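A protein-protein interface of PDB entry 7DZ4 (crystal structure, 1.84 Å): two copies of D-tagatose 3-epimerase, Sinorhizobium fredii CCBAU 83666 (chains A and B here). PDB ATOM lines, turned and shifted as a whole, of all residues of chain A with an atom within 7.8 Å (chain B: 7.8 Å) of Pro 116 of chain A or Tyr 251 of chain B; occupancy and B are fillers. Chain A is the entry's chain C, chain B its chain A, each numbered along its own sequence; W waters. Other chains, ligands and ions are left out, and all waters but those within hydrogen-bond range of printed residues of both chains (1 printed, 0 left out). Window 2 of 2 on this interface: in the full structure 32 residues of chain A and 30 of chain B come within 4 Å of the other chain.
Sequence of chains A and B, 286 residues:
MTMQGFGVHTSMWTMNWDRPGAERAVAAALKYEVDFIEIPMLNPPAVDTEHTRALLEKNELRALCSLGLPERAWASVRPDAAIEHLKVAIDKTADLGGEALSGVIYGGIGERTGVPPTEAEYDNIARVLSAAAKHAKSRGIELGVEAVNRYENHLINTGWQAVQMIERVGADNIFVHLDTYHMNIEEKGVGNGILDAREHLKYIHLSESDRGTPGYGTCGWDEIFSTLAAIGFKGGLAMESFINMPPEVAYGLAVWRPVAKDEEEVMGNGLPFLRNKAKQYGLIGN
Of the printed residues of chain B, Arg 112 of chain A touches Gly 252 and Trp 256. Thr 113 of chain A touches none of the printed residues of chain B. Of the printed residues of chain B, Val 115 of chain A touches Trp 256. Pro 116 of chain A touches two residues of chain B. Of chain B, only Trp 256 (3.9 Å) comes within 4 Å of Pro 117 of chain A. Of the printed residues of chain B, His 154 of chain A touches Trp 256 (3.5 Å). Pro 246 of chain B touches none of the printed residues of chain A. Ala 250 of chain B touches none of the printed residues of chain A. Printed residues of chain A within 4 Å of Tyr 251 of chain B: Gly 114 and Pro 116. Of the printed residues of chain A, Gly 252 of chain B touches Arg 112 (3.9 Å). Printed residues of chain A within 4 Å of Trp 256 of chain B: Arg 112 (3.6 Å), Gly 114 (3.8 Å), Val 115 (3.9 Å), Pro 116 (3.6 Å), Pro 117 (3.9 Å) and His 154 (3.5 Å). The nearest printed residue of chain A that does not touch Tyr 251 of chain B is Val 115 of chain A (4.01 Å).
No position is printed for both chains.
Gly 252 of chain B touches Arg 112 of chain A (O to NH1, 3.9 Å). Trp 256 of chain B touches Arg 112 of chain A (CZ2 to CG, 3.6 Å). Gly 114 of chain A touches Tyr 251 of chain B (O to CB, 3.1 Å). Gly 114 of chain A touches Trp 256 of chain B (C to CZ3, 3.8 Å). Val 115 of chain A touches Trp 256 of chain B (C to CE3, 3.9 Å). Tyr 251 of chain B touches Pro 116 of chain A (CE1 to CG, 3.3 Å). O of Trp 256 of chain B touches CB of Pro 116 of chain A (3.6 Å). O of Trp 256 of chain B touches CD of Pro 117 of chain A, at 3.9 Å. NE1 of Trp 256 of chain B touches CB of His 154 of chain A, 3.5 Å away.
Of the 12 printed residues of chain A, 6 touch a printed residue of chain B. Hydrophobic or aromatic side chains of chain A that line the printed part of chain B: Pro 116, Pro 117 and His 154. Among the printed residues, 9 pairs touch across the chains.
The side-chain hydroxyl (OG1) of Thr 113 of chain A is in hydrogen-bond range of the backbone carbonyl oxygen (O) of Val 115 of chain A, 2.9 Å away. The side-chain carboxylate of Glu 121 of chain A lies within hydrogen-bond range of a ring nitrogen (NE2) of His 154 of chain A, at 2.8 Å.
Water W1 bridges O of Tyr 251 of chain B (2.7 Å) and NH1 of Arg 112 of chain A (2.9 Å).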
ATOM      1  N   ARG A 112      -3.171   0.535  38.611  1.00  0.00           N
ATOM      2  CA  ARG A 112      -2.552   0.887  37.346  1.00  0.00           C
ATOM      3  C   ARG A 112      -1.358  -0.021  37.173  1.00  0.00           C
ATOM      4  O   ARG A 112      -0.552  -0.120  38.097  1.00  0.00           O
ATOM      5  CB  ARG A 112      -2.083   2.347  37.388  1.00  0.00           C
ATOM      6  CG  ARG A 112      -1.560   2.836  36.126  1.00  0.00           C
ATOM      7  CD  ARG A 112      -0.674   4.066  36.304  1.00  0.00           C
ATOM      8  NE  ARG A 112      -1.413   5.279  36.639  1.00  0.00           N
ATOM      9  CZ  ARG A 112      -1.362   6.443  35.976  1.00  0.00           C
ATOM     10  NH1 ARG A 112      -0.627   6.611  34.878  1.00  0.00           N
ATOM     11  NH2 ARG A 112      -2.073   7.471  36.422  1.00  0.00           N
ATOM     12  N   THR A 113      -1.236  -0.666  36.008  1.00  0.00           N
ATOM     13  CA  THR A 113      -0.043  -1.447  35.716  1.00  0.00           C
ATOM     14  C   THR A 113       1.024  -0.621  35.012  1.00  0.00           C
ATOM     15  O   THR A 113       2.203  -1.019  34.983  1.00  0.00           O
ATOM     16  CB  THR A 113      -0.381  -2.654  34.827  1.00  0.00           C
ATOM     17  OG1 THR A 113      -0.991  -2.187  33.613  1.00  0.00           O
ATOM     18  CG2 THR A 113      -1.319  -3.639  35.525  1.00  0.00           C
ATOM     19  N   GLY A 114       0.618   0.494  34.411  1.00  0.00           N
ATOM     20  CA  GLY A 114       1.461   1.280  33.547  1.00  0.00           C
ATOM     21  C   GLY A 114       1.243   1.012  32.078  1.00  0.00           C
ATOM     22  O   GLY A 114       1.752   1.770  31.249  1.00  0.00           O
ATOM     23  N   VAL A 115       0.512  -0.044  31.733  1.00  0.00           N
ATOM     24  CA  VAL A 115       0.221  -0.380  30.341  1.00  0.00           C
ATOM     25  C   VAL A 115      -1.270  -0.686  30.216  1.00  0.00           C
ATOM     26  O   VAL A 115      -1.989  -0.896  31.206  1.00  0.00           O
ATOM     27  CB  VAL A 115       1.082  -1.572  29.852  1.00  0.00           C
ATOM     28  CG1 VAL A 115       2.557  -1.245  29.971  1.00  0.00           C
ATOM     29  CG2 VAL A 115       0.759  -2.837  30.645  1.00  0.00           C
ATOM     30  N   PRO A 116      -1.771  -0.705  28.971  1.00  0.00           N
ATOM     31  CA  PRO A 116      -3.191  -0.963  28.775  1.00  0.00           C
ATOM     32  C   PRO A 116      -3.599  -2.301  29.350  1.00  0.00           C
ATOM     33  O   PRO A 116      -2.779  -3.237  29.497  1.00  0.00           O
ATOM     34  CB  PRO A 116      -3.338  -0.955  27.247  1.00  0.00           C
ATOM     35  CG  PRO A 116      -2.266  -0.047  26.803  1.00  0.00           C
ATOM     36  CD  PRO A 116      -1.105  -0.270  27.741  1.00  0.00           C
ATOM     37  N   PRO A 117      -4.875  -2.460  29.707  1.00  0.00           N
ATOM     38  CA  PRO A 117      -5.372  -3.716  30.265  1.00  0.00           C
ATOM     39  C   PRO A 117      -5.267  -4.862  29.278  1.00  0.00           C
ATOM     40  O   PRO A 117      -5.445  -4.680  28.076  1.00  0.00           O
ATOM     41  CB  PRO A 117      -6.837  -3.412  30.591  1.00  0.00           C
ATOM     42  CG  PRO A 117      -7.208  -2.298  29.633  1.00  0.00           C
ATOM     43  CD  PRO A 117      -5.957  -1.453  29.534  1.00  0.00           C
ATOM     44  N   THR A 118      -5.005  -6.053  29.810  1.00  0.00           N
ATOM     45  CA  THR A 118      -4.822  -7.243  28.994  1.00  0.00           C
ATOM     46  C   THR A 118      -5.978  -8.217  29.170  1.00  0.00           C
ATOM     47  O   THR A 118      -6.734  -8.162  30.143  1.00  0.00           O
ATOM     48  CB  THR A 118      -3.522  -7.981  29.362  1.00  0.00           C
ATOM     49  OG1 THR A 118      -3.658  -8.454  30.705  1.00  0.00           O
ATOM     50  CG2 THR A 118      -2.315  -7.082  29.244  1.00  0.00           C
ATOM     51  N   GLU A 119      -6.072  -9.162  28.227  1.00  0.00           N
ATOM     52  CA  GLU A 119      -7.088 -10.199  28.336  1.00  0.00           C
ATOM     53  C   GLU A 119      -6.848 -11.075  29.557  1.00  0.00           C
ATOM     54  O   GLU A 119      -7.802 -11.572  30.160  1.00  0.00           O
ATOM     55  CB  GLU A 119      -7.110 -11.047  27.063  1.00  0.00           C
ATOM     56  CG  GLU A 119      -8.057 -10.513  25.989  1.00  0.00           C
ATOM     57  CD  GLU A 119      -9.481 -10.402  26.477  1.00  0.00           C
ATOM     58  OE1 GLU A 119      -9.947 -11.323  27.195  1.00  0.00           O
ATOM     59  OE2 GLU A 119     -10.130  -9.382  26.174  1.00  0.00           O
ATOM     60  N   GLU A 121      -5.932 -10.095  32.435  1.00  0.00           N
ATOM     61  CA  GLU A 121      -6.546  -9.380  33.554  1.00  0.00           C
ATOM     62  C   GLU A 121      -8.066  -9.480  33.513  1.00  0.00           C
ATOM     63  O   GLU A 121      -8.711  -9.744  34.537  1.00  0.00           O
ATOM     64  CB  GLU A 121      -6.114  -7.922  33.533  1.00  0.00           C
ATOM     65  CG  GLU A 121      -4.635  -7.740  33.752  1.00  0.00           C
ATOM     66  CD  GLU A 121      -4.181  -6.307  33.549  1.00  0.00           C
ATOM     67  OE1 GLU A 121      -4.048  -5.871  32.383  1.00  0.00           O
ATOM     68  OE2 GLU A 121      -3.941  -5.620  34.572  1.00  0.00           O
ATOM     69  N   TYR A 122      -8.661  -9.277  32.331  1.00  0.00           N
ATOM     70  CA  TYR A 122     -10.109  -9.358  32.235  1.00  0.00           C
ATOM     71  C   TYR A 122     -10.605 -10.760  32.503  1.00  0.00           C
ATOM     72  O   TYR A 122     -11.745 -10.940  32.943  1.00  0.00           O
ATOM     73  CB  TYR A 122     -10.615  -8.929  30.849  1.00  0.00           C
ATOM     74  CG  TYR A 122     -10.500  -7.452  30.627  1.00  0.00           C
ATOM     75  CD1 TYR A 122     -11.169  -6.548  31.452  1.00  0.00           C
ATOM     76  CD2 TYR A 122      -9.737  -6.954  29.585  1.00  0.00           C
ATOM     77  CE1 TYR A 122     -11.056  -5.184  31.251  1.00  0.00           C
ATOM     78  CE2 TYR A 122      -9.610  -5.593  29.373  1.00  0.00           C
ATOM     79  CZ  TYR A 122     -10.297  -4.705  30.197  1.00  0.00           C
ATOM     80  OH  TYR A 122     -10.172  -3.351  29.978  1.00  0.00           O
ATOM     81  N   HIS A 154      -7.292   1.058  35.433  1.00  0.00           N
ATOM     82  CA  HIS A 154      -6.989   0.968  34.011  1.00  0.00           C
ATOM     83  C   HIS A 154      -7.873  -0.019  33.272  1.00  0.00           C
ATOM     84  O   HIS A 154      -7.736  -0.155  32.061  1.00  0.00           O
ATOM     85  CB  HIS A 154      -5.527   0.572  33.791  1.00  0.00           C
ATOM     86  CG  HIS A 154      -5.193  -0.799  34.290  1.00  0.00           C
ATOM     87  ND1 HIS A 154      -5.400  -1.186  35.594  1.00  0.00           N
ATOM     88  CD2 HIS A 154      -4.640  -1.862  33.667  1.00  0.00           C
ATOM     89  CE1 HIS A 154      -5.011  -2.438  35.747  1.00  0.00           C
ATOM     90  NE2 HIS A 154      -4.528  -2.864  34.595  1.00  0.00           N
ATOM     91  N   LEU A 155      -8.802  -0.680  33.958  1.00  0.00           N
ATOM     92  CA  LEU A 155      -9.529  -1.814  33.388  1.00  0.00           C
ATOM     93  C   LEU A 155     -10.934  -1.486  32.878  1.00  0.00           C
ATOM     94  O   LEU A 155     -11.309  -1.933  31.791  1.00  0.00           O
ATOM     95  CB  LEU A 155      -9.599  -2.918  34.443  1.00  0.00           C
ATOM     96  CG  LEU A 155      -8.240  -3.489  34.870  1.00  0.00           C
ATOM     97  CD1 LEU A 155      -8.279  -3.943  36.354  1.00  0.00           C
ATOM     98  CD2 LEU A 155      -7.890  -4.636  33.940  1.00  0.00           C
ATOM     99  N   ILE B 109       4.863  14.493  36.179  1.00  0.00           N
ATOM    100  CA  ILE B 109       3.705  13.610  36.104  1.00  0.00           C
ATOM    101  C   ILE B 109       4.002  12.371  36.942  1.00  0.00           C
ATOM    102  O   ILE B 109       5.039  11.706  36.775  1.00  0.00           O
ATOM    103  CB  ILE B 109       3.359  13.278  34.640  1.00  0.00           C
ATOM    104  CG1 ILE B 109       2.904  14.550  33.903  1.00  0.00           C
ATOM    105  CG2 ILE B 109       2.227  12.229  34.603  1.00  0.00           C
ATOM    106  CD1 ILE B 109       3.556  14.823  32.506  1.00  0.00           C
ATOM    107  N   MET B 245       0.017   9.438  19.762  1.00  0.00           N
ATOM    108  CA  MET B 245       1.183   9.540  20.638  1.00  0.00           C
ATOM    109  C   MET B 245       1.938   8.212  20.628  1.00  0.00           C
ATOM    110  O   MET B 245       1.315   7.141  20.543  1.00  0.00           O
ATOM    111  CB  MET B 245       0.805   9.901  22.071  1.00  0.00           C
ATOM    112  CG  MET B 245       1.789  10.961  22.718  1.00  0.00           C
ATOM    113  SD  MET B 245       0.941  12.006  23.935  1.00  0.00           S
ATOM    114  CE  MET B 245       0.276  10.634  24.845  1.00  0.00           C
ATOM    115  N   PRO B 246       3.267   8.242  20.703  1.00  0.00           N
ATOM    116  CA  PRO B 246       4.032   6.999  20.914  1.00  0.00           C
ATOM    117  C   PRO B 246       3.527   6.262  22.136  1.00  0.00           C
ATOM    118  O   PRO B 246       3.344   6.877  23.191  1.00  0.00           O
ATOM    119  CB  PRO B 246       5.475   7.491  21.133  1.00  0.00           C
ATOM    120  CG  PRO B 246       5.536   8.842  20.504  1.00  0.00           C
ATOM    121  CD  PRO B 246       4.138   9.436  20.660  1.00  0.00           C
ATOM    122  N   PRO B 247       3.335   4.943  22.047  1.00  0.00           N
ATOM    123  CA  PRO B 247       2.721   4.220  23.176  1.00  0.00           C
ATOM    124  C   PRO B 247       3.327   4.506  24.536  1.00  0.00           C
ATOM    125  O   PRO B 247       2.573   4.827  25.468  1.00  0.00           O
ATOM    126  CB  PRO B 247       2.891   2.755  22.755  1.00  0.00           C
ATOM    127  CG  PRO B 247       2.694   2.826  21.246  1.00  0.00           C
ATOM    128  CD  PRO B 247       3.418   4.099  20.837  1.00  0.00           C
ATOM    129  N   GLU B 248       4.655   4.419  24.681  1.00  0.00           N
ATOM    130  CA  GLU B 248       5.260   4.565  26.006  1.00  0.00           C
ATOM    131  C   GLU B 248       4.881   5.899  26.638  1.00  0.00           C
ATOM    132  O   GLU B 248       4.579   5.969  27.840  1.00  0.00           O
ATOM    133  CB  GLU B 248       6.788   4.440  25.926  1.00  0.00           C
ATOM    134  CG  GLU B 248       7.476   4.195  27.285  1.00  0.00           C
ATOM    135  CD  GLU B 248       8.642   5.159  27.578  1.00  0.00           C
ATOM    136  OE1 GLU B 248       9.635   4.722  28.226  1.00  0.00           O
ATOM    137  OE2 GLU B 248       8.561   6.347  27.169  1.00  0.00           O
ATOM    138  N   VAL B 249       4.901   6.971  25.840  1.00  0.00           N
ATOM    139  CA  VAL B 249       4.469   8.266  26.340  1.00  0.00           C
ATOM    140  C   VAL B 249       2.991   8.223  26.698  1.00  0.00           C
ATOM    141  O   VAL B 249       2.578   8.744  27.737  1.00  0.00           O
ATOM    142  CB  VAL B 249       4.758   9.367  25.295  1.00  0.00           C
ATOM    143  CG1 VAL B 249       4.086  10.692  25.725  1.00  0.00           C
ATOM    144  CG2 VAL B 249       6.276   9.523  25.057  1.00  0.00           C
ATOM    145  N   ALA B 250       2.168   7.632  25.820  1.00  0.00           N
ATOM    146  CA  ALA B 250       0.727   7.571  26.057  1.00  0.00           C
ATOM    147  C   ALA B 250       0.422   6.807  27.334  1.00  0.00           C
ATOM    148  O   ALA B 250      -0.394   7.249  28.147  1.00  0.00           O
ATOM    149  CB  ALA B 250       0.026   6.917  24.861  1.00  0.00           C
ATOM    150  N   TYR B 251       1.088   5.666  27.547  1.00  0.00           N
ATOM    151  CA  TYR B 251       0.822   4.888  28.756  1.00  0.00           C
ATOM    152  C   TYR B 251       1.157   5.693  30.007  1.00  0.00           C
ATOM    153  O   TYR B 251       0.430   5.636  31.001  1.00  0.00           O
ATOM    154  CB  TYR B 251       1.625   3.589  28.732  1.00  0.00           C
ATOM    155  CG  TYR B 251       1.376   2.690  27.533  1.00  0.00           C
ATOM    156  CD1 TYR B 251       0.268   2.862  26.703  1.00  0.00           C
ATOM    157  CD2 TYR B 251       2.263   1.667  27.230  1.00  0.00           C
ATOM    158  CE1 TYR B 251       0.044   2.013  25.620  1.00  0.00           C
ATOM    159  CE2 TYR B 251       2.056   0.838  26.156  1.00  0.00           C
ATOM    160  CZ  TYR B 251       0.953   1.007  25.352  1.00  0.00           C
ATOM    161  OH  TYR B 251       0.771   0.148  24.283  1.00  0.00           O
ATOM    162  N   GLY B 252       2.255   6.458  29.969  1.00  0.00           N
ATOM    163  CA  GLY B 252       2.615   7.322  31.071  1.00  0.00           C
ATOM    164  C   GLY B 252       1.586   8.383  31.391  1.00  0.00           C
ATOM    165  O   GLY B 252       1.572   8.886  32.529  1.00  0.00           O
ATOM    166  N   LEU B 253       0.724   8.732  30.411  1.00  0.00           N
ATOM    167  CA  LEU B 253      -0.370   9.693  30.551  1.00  0.00           C
ATOM    168  C   LEU B 253      -1.739   9.025  30.723  1.00  0.00           C
ATOM    169  O   LEU B 253      -2.791   9.671  30.550  1.00  0.00           O
ATOM    170  CB  LEU B 253      -0.404  10.595  29.326  1.00  0.00           C
ATOM    171  CG  LEU B 253       0.729  11.627  29.382  1.00  0.00           C
ATOM    172  CD1 LEU B 253       1.156  11.994  27.978  1.00  0.00           C
ATOM    173  CD2 LEU B 253       0.243  12.828  30.161  1.00  0.00           C
ATOM    174  N   ALA B 254      -1.745   7.752  31.056  1.00  0.00           N
ATOM    175  CA  ALA B 254      -2.965   7.001  31.353  1.00  0.00           C
ATOM    176  C   ALA B 254      -3.856   6.830  30.128  1.00  0.00           C
ATOM    177  O   ALA B 254      -5.057   6.680  30.249  1.00  0.00           O
ATOM    178  CB  ALA B 254      -3.764   7.649  32.479  1.00  0.00           C
ATOM    179  N   VAL B 255      -3.279   6.755  28.944  1.00  0.00           N
ATOM    180  CA  VAL B 255      -4.044   6.429  27.755  1.00  0.00           C
ATOM    181  C   VAL B 255      -4.083   4.914  27.633  1.00  0.00           C
ATOM    182  O   VAL B 255      -3.102   4.275  27.274  1.00  0.00           O
ATOM    183  CB  VAL B 255      -3.460   7.100  26.512  1.00  0.00           C
ATOM    184  CG1 VAL B 255      -4.400   6.900  25.340  1.00  0.00           C
ATOM    185  CG2 VAL B 255      -3.230   8.568  26.823  1.00  0.00           C
ATOM    186  N   TRP B 256      -5.232   4.330  27.930  1.00  0.00           N
ATOM    187  CA  TRP B 256      -5.338   2.882  27.954  1.00  0.00           C
ATOM    188  C   TRP B 256      -6.066   2.332  26.743  1.00  0.00           C
ATOM    189  O   TRP B 256      -6.229   1.112  26.626  1.00  0.00           O
ATOM    190  CB  TRP B 256      -6.046   2.430  29.217  1.00  0.00           C
ATOM    191  CG  TRP B 256      -5.559   3.032  30.526  1.00  0.00           C
ATOM    192  CD1 TRP B 256      -6.342   3.500  31.550  1.00  0.00           C
ATOM    193  CD2 TRP B 256      -4.204   3.124  30.991  1.00  0.00           C
ATOM    194  NE1 TRP B 256      -5.545   3.906  32.619  1.00  0.00           N
ATOM    195  CE2 TRP B 256      -4.233   3.697  32.291  1.00  0.00           C
ATOM    196  CE3 TRP B 256      -2.961   2.803  30.422  1.00  0.00           C
ATOM    197  CZ2 TRP B 256      -3.073   3.961  33.020  1.00  0.00           C
ATOM    198  CZ3 TRP B 256      -1.816   3.054  31.151  1.00  0.00           C
ATOM    199  CH2 TRP B 256      -1.880   3.624  32.437  1.00  0.00           C
ATOM    200  N   ARG B 257      -6.509   3.214  25.861  1.00  0.00           N
ATOM    201  CA  ARG B 257      -7.396   2.919  24.747  1.00  0.00           C
ATOM    202  C   ARG B 257      -7.362   4.120  23.824  1.00  0.00           C
ATOM    203  O   ARG B 257      -6.979   5.213  24.255  1.00  0.00           O
ATOM    204  CB  ARG B 257      -8.836   2.649  25.228  1.00  0.00           C
ATOM    205  CG  ARG B 257      -9.482   3.813  26.002  1.00  0.00           C
ATOM    206  CD  ARG B 257     -10.817   3.416  26.696  1.00  0.00           C
ATOM    207  NE  ARG B 257     -11.350   4.583  27.431  1.00  0.00           N
ATOM    208  CZ  ARG B 257     -12.152   5.523  26.949  1.00  0.00           C
ATOM    209  NH1 ARG B 257     -12.593   5.513  25.679  1.00  0.00           N
ATOM    210  NH2 ARG B 257     -12.518   6.502  27.755  1.00  0.00           N
HETATM  211  O   HOH W   1       1.249   4.926  33.488  1.00  0.00           O
